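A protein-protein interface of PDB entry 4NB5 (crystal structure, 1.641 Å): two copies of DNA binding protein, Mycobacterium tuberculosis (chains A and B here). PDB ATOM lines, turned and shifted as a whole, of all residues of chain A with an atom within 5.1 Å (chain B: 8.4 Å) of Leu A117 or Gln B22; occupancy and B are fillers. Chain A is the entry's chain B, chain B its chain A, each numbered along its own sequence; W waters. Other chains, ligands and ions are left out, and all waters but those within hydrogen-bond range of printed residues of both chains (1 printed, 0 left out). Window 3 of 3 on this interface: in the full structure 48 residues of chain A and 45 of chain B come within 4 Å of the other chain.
Water W1 lies within hydrogen-bond range of O of Val A120 (2.8 Å) and OD1 of Asp B15 (3.1 Å).
No position is printed for both chains.
Among the printed residues, merely in contact across the chains: Leu A114 with Tyr B26 (3.1 Å), Leu A117 with Phe B19 (3.2 Å), Leu A117 with Gln B22 (3.5 Å), Leu A117 with Met B23 (3.9 Å), Leu A117 with Tyr B26 (3.7 Å), Val A120 with Phe B19 (3.98 Å), Val A120 with Gln B22 (3.7 Å) and Gly A121 with Phe B19 (3.6 Å).
Hydrophobic or aromatic side chains of chain A that line the printed part of chain B: Leu A114, Leu A117 and Val A120.
Printed residues of chain B that touch a printed residue of chain A: Phe B19, Gln B22, Met B23 and Tyr B26.
Among the printed residues, no Asp or Glu carboxylate lies within 4 Å of a Lys or Arg side-chain nitrogen of the other chain.
Of chain B, only Phe B19 (3.2 Å), Gln B22 (3.5 Å), Met B23 (3.9 Å) and Tyr B26 (3.7 Å) come within 4 Å of Leu A117.
Of the printed residues of chain B, Leu A114 touches Tyr B26 (3.1 Å).
Of the printed residues of chain B, Gly A121 touches Phe B19 (3.6 Å).
Printed residues of chain B within 4 Å of Val A120: Phe B19 and Gln B22.
Printed residues of chain A within 4 Å of Met B23: Leu A117.
Of the printed residues of chain A, Tyr B26 touches Leu A114 (3.1 Å) and Leu A117 (3.7 Å).
The nearest residue of chain B that does not touch Leu A117 is Gly B25 (6.5 Å).
The nearest printed residue of chain B that does not touch Leu A114 is Met B23 (4.2 Å).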
ATOM      1  N   GLU A 113      -8.199  13.846  15.406  1.00  0.00           N
ATOM      2  CA  GLU A 113      -8.844  12.685  14.810  1.00  0.00           C
ATOM      3  C   GLU A 113     -10.169  12.395  15.506  1.00  0.00           C
ATOM      4  O   GLU A 113     -11.151  12.042  14.860  1.00  0.00           O
ATOM      5  CB  GLU A 113      -7.924  11.469  14.884  1.00  0.00           C
ATOM      6  CG  GLU A 113      -6.691  11.603  14.013  1.00  0.00           C
ATOM      7  CD  GLU A 113      -5.744  10.424  14.130  1.00  0.00           C
ATOM      8  OE1 GLU A 113      -4.802  10.346  13.315  1.00  0.00           O
ATOM      9  OE2 GLU A 113      -5.936   9.579  15.030  1.00  0.00           O
ATOM     10  N   LEU A 114     -10.189  12.549  16.828  1.00  0.00           N
ATOM     11  CA  LEU A 114     -11.414  12.353  17.596  1.00  0.00           C
ATOM     12  C   LEU A 114     -12.449  13.417  17.257  1.00  0.00           C
ATOM     13  O   LEU A 114     -13.646  13.135  17.213  1.00  0.00           O
ATOM     14  CB  LEU A 114     -11.117  12.380  19.096  1.00  0.00           C
ATOM     15  CG  LEU A 114     -10.579  11.077  19.676  1.00  0.00           C
ATOM     16  CD1 LEU A 114     -10.125  11.286  21.114  1.00  0.00           C
ATOM     17  CD2 LEU A 114     -11.638   9.987  19.604  1.00  0.00           C
ATOM     18  N   GLN A 115     -11.990  14.637  16.998  1.00  0.00           N
ATOM     19  CA  GLN A 115     -12.894  15.704  16.620  1.00  0.00           C
ATOM     20  C   GLN A 115     -13.561  15.376  15.285  1.00  0.00           C
ATOM     21  O   GLN A 115     -14.753  15.610  15.100  1.00  0.00           O
ATOM     22  CB  GLN A 115     -12.145  17.036  16.546  1.00  0.00           C
ATOM     23  CG  GLN A 115     -13.070  18.232  16.536  1.00  0.00           C
ATOM     24  CD  GLN A 115     -12.359  19.541  16.252  1.00  0.00           C
ATOM     25  OE1 GLN A 115     -12.948  20.463  15.683  1.00  0.00           O
ATOM     26  NE2 GLN A 115     -11.096  19.635  16.651  1.00  0.00           N
ATOM     27  N   ASP A 116     -12.795  14.818  14.354  1.00  0.00           N
ATOM     28  CA  ASP A 116     -13.348  14.408  13.074  1.00  0.00           C
ATOM     29  C   ASP A 116     -14.378  13.298  13.282  1.00  0.00           C
ATOM     30  O   ASP A 116     -15.403  13.249  12.599  1.00  0.00           O
ATOM     31  CB  ASP A 116     -12.234  13.941  12.129  1.00  0.00           C
ATOM     32  CG  ASP A 116     -11.498  15.102  11.472  1.00  0.00           C
ATOM     33  OD1 ASP A 116     -12.065  16.216  11.403  1.00  0.00           O
ATOM     34  OD2 ASP A 116     -10.346  14.901  11.022  1.00  0.00           O
ATOM     35  N   LEU A 117     -14.107  12.401  14.224  1.00  0.00           N
ATOM     36  CA  LEU A 117     -15.058  11.333  14.519  1.00  0.00           C
ATOM     37  C   LEU A 117     -16.344  11.896  15.115  1.00  0.00           C
ATOM     38  O   LEU A 117     -17.436  11.405  14.829  1.00  0.00           O
ATOM     39  CB  LEU A 117     -14.440  10.274  15.441  1.00  0.00           C
ATOM     40  CG  LEU A 117     -13.350   9.434  14.765  1.00  0.00           C
ATOM     41  CD1 LEU A 117     -12.659   8.500  15.741  1.00  0.00           C
ATOM     42  CD2 LEU A 117     -13.926   8.630  13.601  1.00  0.00           C
ATOM     43  N   ALA A 118     -16.226  12.933  15.936  1.00  0.00           N
ATOM     44  CA  ALA A 118     -17.414  13.533  16.529  1.00  0.00           C
ATOM     45  C   ALA A 118     -18.295  14.091  15.418  1.00  0.00           C
ATOM     46  O   ALA A 118     -19.526  14.014  15.493  1.00  0.00           O
ATOM     47  CB  ALA A 118     -17.043  14.611  17.512  1.00  0.00           C
ATOM     48  N   ASP A 119     -17.666  14.632  14.375  1.00  0.00           N
ATOM     49  CA  ASP A 119     -18.415  15.153  13.230  1.00  0.00           C
ATOM     50  C   ASP A 119     -19.180  14.041  12.499  1.00  0.00           C
ATOM     51  O   ASP A 119     -20.310  14.258  12.044  1.00  0.00           O
ATOM     52  CB  ASP A 119     -17.484  15.879  12.243  1.00  0.00           C
ATOM     53  CG  ASP A 119     -16.954  17.194  12.784  1.00  0.00           C
ATOM     54  OD1 ASP A 119     -17.594  17.790  13.680  1.00  0.00           O
ATOM     55  OD2 ASP A 119     -15.889  17.636  12.299  1.00  0.00           O
ATOM     56  N   VAL A 120     -18.571  12.863  12.389  1.00  0.00           N
ATOM     57  CA  VAL A 120     -19.228  11.699  11.802  1.00  0.00           C
ATOM     58  C   VAL A 120     -20.472  11.369  12.608  1.00  0.00           C
ATOM     59  O   VAL A 120     -21.541  11.115  12.052  1.00  0.00           O
ATOM     60  CB  VAL A 120     -18.307  10.463  11.801  1.00  0.00           C
ATOM     61  CG1 VAL A 120     -19.074   9.195  11.391  1.00  0.00           C
ATOM     62  CG2 VAL A 120     -17.105  10.685  10.884  1.00  0.00           C
ATOM     63  N   GLY A 121     -20.321  11.357  13.929  1.00  0.00           N
ATOM     64  CA  GLY A 121     -21.430  11.043  14.809  1.00  0.00           C
ATOM     65  C   GLY A 121     -22.547  12.065  14.706  1.00  0.00           C
ATOM     66  O   GLY A 121     -23.732  11.706  14.704  1.00  0.00           O
ATOM     67  N   ASP B  15     -26.285   4.332   9.973  1.00  0.00           N
ATOM     68  CA  ASP B  15     -24.965   4.952   9.950  1.00  0.00           C
ATOM     69  C   ASP B  15     -24.444   5.186  11.363  1.00  0.00           C
ATOM     70  O   ASP B  15     -23.294   5.590  11.544  1.00  0.00           O
ATOM     71  CB  ASP B  15     -25.009   6.287   9.202  1.00  0.00           C
ATOM     72  CG  ASP B  15     -23.652   6.696   8.654  1.00  0.00           C
ATOM     73  OD1 ASP B  15     -22.827   7.238   9.421  1.00  0.00           O
ATOM     74  OD2 ASP B  15     -23.411   6.482   7.448  1.00  0.00           O
ATOM     75  N   ILE B  16     -25.294   4.973  12.364  1.00  0.00           N
ATOM     76  CA  ILE B  16     -24.840   5.116  13.740  1.00  0.00           C
ATOM     77  C   ILE B  16     -23.804   4.037  14.012  1.00  0.00           C
ATOM     78  O   ILE B  16     -22.747   4.311  14.584  1.00  0.00           O
ATOM     79  CB  ILE B  16     -25.997   5.041  14.755  1.00  0.00           C
ATOM     80  CG1 ILE B  16     -26.550   6.440  15.025  1.00  0.00           C
ATOM     81  CG2 ILE B  16     -25.541   4.418  16.063  1.00  0.00           C
ATOM     82  CD1 ILE B  16     -25.520   7.420  15.588  1.00  0.00           C
ATOM     83  N   MET B  17     -24.077   2.815  13.566  1.00  0.00           N
ATOM     84  CA  MET B  17     -23.120   1.743  13.780  1.00  0.00           C
ATOM     85  C   MET B  17     -21.804   2.036  13.065  1.00  0.00           C
ATOM     86  O   MET B  17     -20.760   1.525  13.464  1.00  0.00           O
ATOM     87  CB  MET B  17     -23.684   0.376  13.375  1.00  0.00           C
ATOM     88  CG  MET B  17     -24.546  -0.283  14.453  1.00  0.00           C
ATOM     89  SD  MET B  17     -23.844  -0.244  16.134  1.00  0.00           S
ATOM     90  CE  MET B  17     -22.217  -0.936  15.859  1.00  0.00           C
ATOM     91  N   GLU B  18     -21.834   2.879  12.034  1.00  0.00           N
ATOM     92  CA  GLU B  18     -20.595   3.268  11.356  1.00  0.00           C
ATOM     93  C   GLU B  18     -19.709   4.121  12.274  1.00  0.00           C
ATOM     94  O   GLU B  18     -18.508   3.870  12.404  1.00  0.00           O
ATOM     95  CB  GLU B  18     -20.888   4.013  10.050  1.00  0.00           C
ATOM     96  CG  GLU B  18     -21.736   3.227   9.051  1.00  0.00           C
ATOM     97  CD  GLU B  18     -21.070   1.948   8.544  1.00  0.00           C
ATOM     98  OE1 GLU B  18     -19.885   1.697   8.861  1.00  0.00           O
ATOM     99  OE2 GLU B  18     -21.745   1.183   7.820  1.00  0.00           O
ATOM    100  N   PHE B  19     -20.298   5.115  12.930  1.00  0.00           N
ATOM    101  CA  PHE B  19     -19.550   5.933  13.880  1.00  0.00           C
ATOM    102  C   PHE B  19     -19.006   5.060  15.018  1.00  0.00           C
ATOM    103  O   PHE B  19     -17.852   5.192  15.421  1.00  0.00           O
ATOM    104  CB  PHE B  19     -20.446   7.039  14.444  1.00  0.00           C
ATOM    105  CG  PHE B  19     -19.919   7.664  15.700  1.00  0.00           C
ATOM    106  CD1 PHE B  19     -18.897   8.590  15.663  1.00  0.00           C
ATOM    107  CD2 PHE B  19     -20.452   7.321  16.928  1.00  0.00           C
ATOM    108  CE1 PHE B  19     -18.413   9.163  16.831  1.00  0.00           C
ATOM    109  CE2 PHE B  19     -19.975   7.882  18.091  1.00  0.00           C
ATOM    110  CZ  PHE B  19     -18.962   8.797  18.053  1.00  0.00           C
ATOM    111  N   VAL B  20     -19.851   4.173  15.527  1.00  0.00           N
ATOM    112  CA  VAL B  20     -19.441   3.270  16.602  1.00  0.00           C
ATOM    113  C   VAL B  20     -18.242   2.431  16.165  1.00  0.00           C
ATOM    114  O   VAL B  20     -17.257   2.309  16.895  1.00  0.00           O
ATOM    115  CB  VAL B  20     -20.609   2.362  17.027  1.00  0.00           C
ATOM    116  CG1 VAL B  20     -20.147   1.280  18.012  1.00  0.00           C
ATOM    117  CG2 VAL B  20     -21.723   3.204  17.626  1.00  0.00           C
ATOM    118  N   GLU B  21     -18.314   1.873  14.963  1.00  0.00           N
ATOM    119  CA  GLU B  21     -17.236   1.026  14.469  1.00  0.00           C
ATOM    120  C   GLU B  21     -15.953   1.832  14.315  1.00  0.00           C
ATOM    121  O   GLU B  21     -14.861   1.340  14.604  1.00  0.00           O
ATOM    122  CB  GLU B  21     -17.632   0.383  13.134  1.00  0.00           C
ATOM    123  CG  GLU B  21     -16.976  -0.964  12.888  1.00  0.00           C
ATOM    124  CD  GLU B  21     -17.225  -1.944  14.024  1.00  0.00           C
ATOM    125  OE1 GLU B  21     -16.317  -2.745  14.324  1.00  0.00           O
ATOM    126  OE2 GLU B  21     -18.323  -1.911  14.617  1.00  0.00           O
ATOM    127  N   GLN B  22     -16.087   3.086  13.883  1.00  0.00           N
ATOM    128  CA  GLN B  22     -14.927   3.952  13.705  1.00  0.00           C
ATOM    129  C   GLN B  22     -14.274   4.306  15.038  1.00  0.00           C
ATOM    130  O   GLN B  22     -13.051   4.429  15.123  1.00  0.00           O
ATOM    131  CB  GLN B  22     -15.304   5.219  12.921  1.00  0.00           C
ATOM    132  CG  GLN B  22     -15.661   4.931  11.455  1.00  0.00           C
ATOM    133  CD  GLN B  22     -16.119   6.168  10.687  1.00  0.00           C
ATOM    134  OE1 GLN B  22     -15.609   7.265  10.897  1.00  0.00           O
ATOM    135  NE2 GLN B  22     -17.089   5.987   9.791  1.00  0.00           N
ATOM    136  N   MET B  23     -15.075   4.462  16.087  1.00  0.00           N
ATOM    137  CA  MET B  23     -14.513   4.696  17.411  1.00  0.00           C
ATOM    138  C   MET B  23     -13.755   3.453  17.894  1.00  0.00           C
ATOM    139  O   MET B  23     -12.739   3.571  18.583  1.00  0.00           O
ATOM    140  CB  MET B  23     -15.604   5.077  18.413  1.00  0.00           C
ATOM    141  CG  MET B  23     -16.175   6.472  18.182  1.00  0.00           C
ATOM    142  SD  MET B  23     -15.089   7.797  18.731  1.00  0.00           S
ATOM    143  CE  MET B  23     -15.097   7.517  20.503  1.00  0.00           C
ATOM    144  N   GLY B  24     -14.251   2.275  17.540  1.00  0.00           N
ATOM    145  CA  GLY B  24     -13.541   1.044  17.852  1.00  0.00           C
ATOM    146  C   GLY B  24     -12.171   1.063  17.196  1.00  0.00           C
ATOM    147  O   GLY B  24     -11.170   0.675  17.791  1.00  0.00           O
ATOM    148  N   GLY B  25     -12.132   1.536  15.956  1.00  0.00           N
ATOM    149  CA  GLY B  25     -10.885   1.666  15.207  1.00  0.00           C
ATOM    150  C   GLY B  25      -9.893   2.637  15.813  1.00  0.00           C
ATOM    151  O   GLY B  25      -8.692   2.353  15.888  1.00  0.00           O
ATOM    152  N   TYR B  26     -10.382   3.795  16.239  1.00  0.00           N
ATOM    153  CA  TYR B  26      -9.537   4.773  16.905  1.00  0.00           C
ATOM    154  C   TYR B  26      -8.906   4.146  18.139  1.00  0.00           C
ATOM    155  O   TYR B  26      -7.720   4.329  18.397  1.00  0.00           O
ATOM    156  CB  TYR B  26     -10.339   6.018  17.289  1.00  0.00           C
ATOM    157  CG  TYR B  26      -9.584   6.995  18.161  1.00  0.00           C
ATOM    158  CD1 TYR B  26      -8.781   7.983  17.602  1.00  0.00           C
ATOM    159  CD2 TYR B  26      -9.678   6.940  19.542  1.00  0.00           C
ATOM    160  CE1 TYR B  26      -8.092   8.877  18.397  1.00  0.00           C
ATOM    161  CE2 TYR B  26      -8.994   7.829  20.345  1.00  0.00           C
ATOM    162  CZ  TYR B  26      -8.201   8.795  19.768  1.00  0.00           C
ATOM    163  OH  TYR B  26      -7.523   9.677  20.575  1.00  0.00           O
ATOM    164  N   PHE B  27      -9.689   3.394  18.905  1.00  0.00           N
ATOM    165  CA  PHE B  27      -9.130   2.775  20.094  1.00  0.00           C
ATOM    166  C   PHE B  27      -8.085   1.720  19.729  1.00  0.00           C
ATOM    167  O   PHE B  27      -6.999   1.689  20.311  1.00  0.00           O
ATOM    168  CB  PHE B  27     -10.227   2.187  20.988  1.00  0.00           C
ATOM    169  CG  PHE B  27     -10.747   3.159  22.006  1.00  0.00           C
ATOM    170  CD1 PHE B  27     -11.285   4.373  21.599  1.00  0.00           C
ATOM    171  CD2 PHE B  27     -10.704   2.866  23.356  1.00  0.00           C
ATOM    172  CE1 PHE B  27     -11.762   5.277  22.521  1.00  0.00           C
ATOM    173  CE2 PHE B  27     -11.178   3.766  24.288  1.00  0.00           C
ATOM    174  CZ  PHE B  27     -11.711   4.977  23.869  1.00  0.00           C
ATOM    175  N   GLU B  28      -8.408   0.867  18.767  1.00  0.00           N
ATOM    176  CA  GLU B  28      -7.511  -0.229  18.417  1.00  0.00           C
ATOM    177  C   GLU B  28      -6.203   0.293  17.832  1.00  0.00           C
ATOM    178  O   GLU B  28      -5.165  -0.358  17.959  1.00  0.00           O
ATOM    179  CB  GLU B  28      -8.181  -1.198  17.445  1.00  0.00           C
ATOM    180  CG  GLU B  28      -7.394  -2.476  17.234  1.00  0.00           C
ATOM    181  CD  GLU B  28      -8.252  -3.597  16.699  1.00  0.00           C
ATOM    182  OE1 GLU B  28      -9.295  -3.296  16.084  1.00  0.00           O
ATOM    183  OE2 GLU B  28      -7.892  -4.776  16.897  1.00  0.00           O
ATOM    184  N   SER B  29      -6.255   1.467  17.207  1.00  0.00           N
ATOM    185  CA  SER B  29      -5.064   2.074  16.621  1.00  0.00           C
ATOM    186  C   SER B  29      -4.118   2.593  17.698  1.00  0.00           C
ATOM    187  O   SER B  29      -2.905   2.649  17.496  1.00  0.00           O
ATOM    188  CB  SER B  29      -5.454   3.211  15.673  1.00  0.00           C
ATOM    189  OG  SER B  29      -6.089   2.708  14.510  1.00  0.00           O
ATOM    190  N   ARG B  34     -10.861  -2.711  20.837  1.00  0.00           N
ATOM    191  CA  ARG B  34     -11.838  -2.266  19.916  1.00  0.00           C
ATOM    192  C   ARG B  34     -13.171  -2.108  20.671  1.00  0.00           C
ATOM    193  O   ARG B  34     -13.913  -1.233  20.416  1.00  0.00           O
ATOM    194  CB  ARG B  34     -12.020  -3.320  18.854  1.00  0.00           C
ATOM    195  CG  ARG B  34     -13.107  -3.038  17.849  1.00  0.00           C
ATOM    196  CD  ARG B  34     -13.066  -3.965  16.649  1.00  0.00           C
ATOM    197  NE  ARG B  34     -12.250  -3.327  15.626  1.00  0.00           N
ATOM    198  CZ  ARG B  34     -12.551  -2.172  14.994  1.00  0.00           C
ATOM    199  NH1 ARG B  34     -13.724  -1.420  15.232  1.00  0.00           N
ATOM    200  NH2 ARG B  34     -11.655  -1.729  14.125  1.00  0.00           N
ATOM    201  N   GLY B  37     -13.607   1.167  22.575  1.00  0.00           N
ATOM    202  CA  GLY B  37     -13.931   2.225  21.636  1.00  0.00           C
ATOM    203  C   GLY B  37     -15.375   2.189  21.175  1.00  0.00           C
ATOM    204  O   GLY B  37     -16.046   3.225  21.123  1.00  0.00           O
ATOM    205  N   ARG B  38     -15.857   0.999  20.830  1.00  0.00           N
ATOM    206  CA  ARG B  38     -17.238   0.847  20.406  1.00  0.00           C
ATOM    207  C   ARG B  38     -18.185   1.211  21.544  1.00  0.00           C
ATOM    208  O   ARG B  38     -19.249   1.802  21.322  1.00  0.00           O
ATOM    209  CB  ARG B  38     -17.499  -0.581  19.915  1.00  0.00           C
ATOM    210  CG  ARG B  38     -16.720  -0.934  18.654  1.00  0.00           C
ATOM    211  CD  ARG B  38     -16.989  -2.340  18.174  1.00  0.00           C
ATOM    212  NE  ARG B  38     -18.368  -2.501  17.735  1.00  0.00           N
ATOM    213  CZ  ARG B  38     -19.206  -3.438  18.176  1.00  0.00           C
ATOM    214  NH1 ARG B  38     -18.827  -4.333  19.080  1.00  0.00           N
ATOM    215  NH2 ARG B  38     -20.440  -3.474  17.702  1.00  0.00           N
ATOM    216  N   GLY B  41     -18.197   4.964  21.911  1.00  0.00           N
ATOM    217  CA  GLY B  41     -18.981   5.455  20.785  1.00  0.00           C
ATOM    218  C   GLY B  41     -20.472   5.296  21.012  1.00  0.00           C
ATOM    219  O   GLY B  41     -21.252   6.240  20.824  1.00  0.00           O
ATOM    220  N   LEU B  44     -21.916   7.666  23.472  1.00  0.00           N
ATOM    221  CA  LEU B  44     -21.955   9.030  22.956  1.00  0.00           C
ATOM    222  C   LEU B  44     -23.220   9.307  22.146  1.00  0.00           C
ATOM    223  O   LEU B  44     -23.621  10.461  22.009  1.00  0.00           O
ATOM    224  CB  LEU B  44     -20.735   9.308  22.085  1.00  0.00           C
ATOM    225  CG  LEU B  44     -19.494   9.682  22.882  1.00  0.00           C
ATOM    226  CD1 LEU B  44     -18.219   9.411  22.097  1.00  0.00           C
ATOM    227  CD2 LEU B  44     -19.568  11.143  23.288  1.00  0.00           C
ATOM    228  N   VAL B  45     -23.845   8.262  21.605  1.00  0.00           N
ATOM    229  CA  VAL B  45     -24.951   8.465  20.664  1.00  0.00           C
ATOM    230  C   VAL B  45     -26.258   7.771  21.030  1.00  0.00           C
ATOM    231  O   VAL B  45     -27.299   8.040  20.416  1.00  0.00           O
ATOM    232  CB  VAL B  45     -24.564   8.019  19.230  1.00  0.00           C
ATOM    233  CG1 VAL B  45     -23.387   8.834  18.725  1.00  0.00           C
ATOM    234  CG2 VAL B  45     -24.261   6.529  19.186  1.00  0.00           C
HETATM  235  O   HOH W   1     -21.907  10.245   9.417  1.00  0.00           O
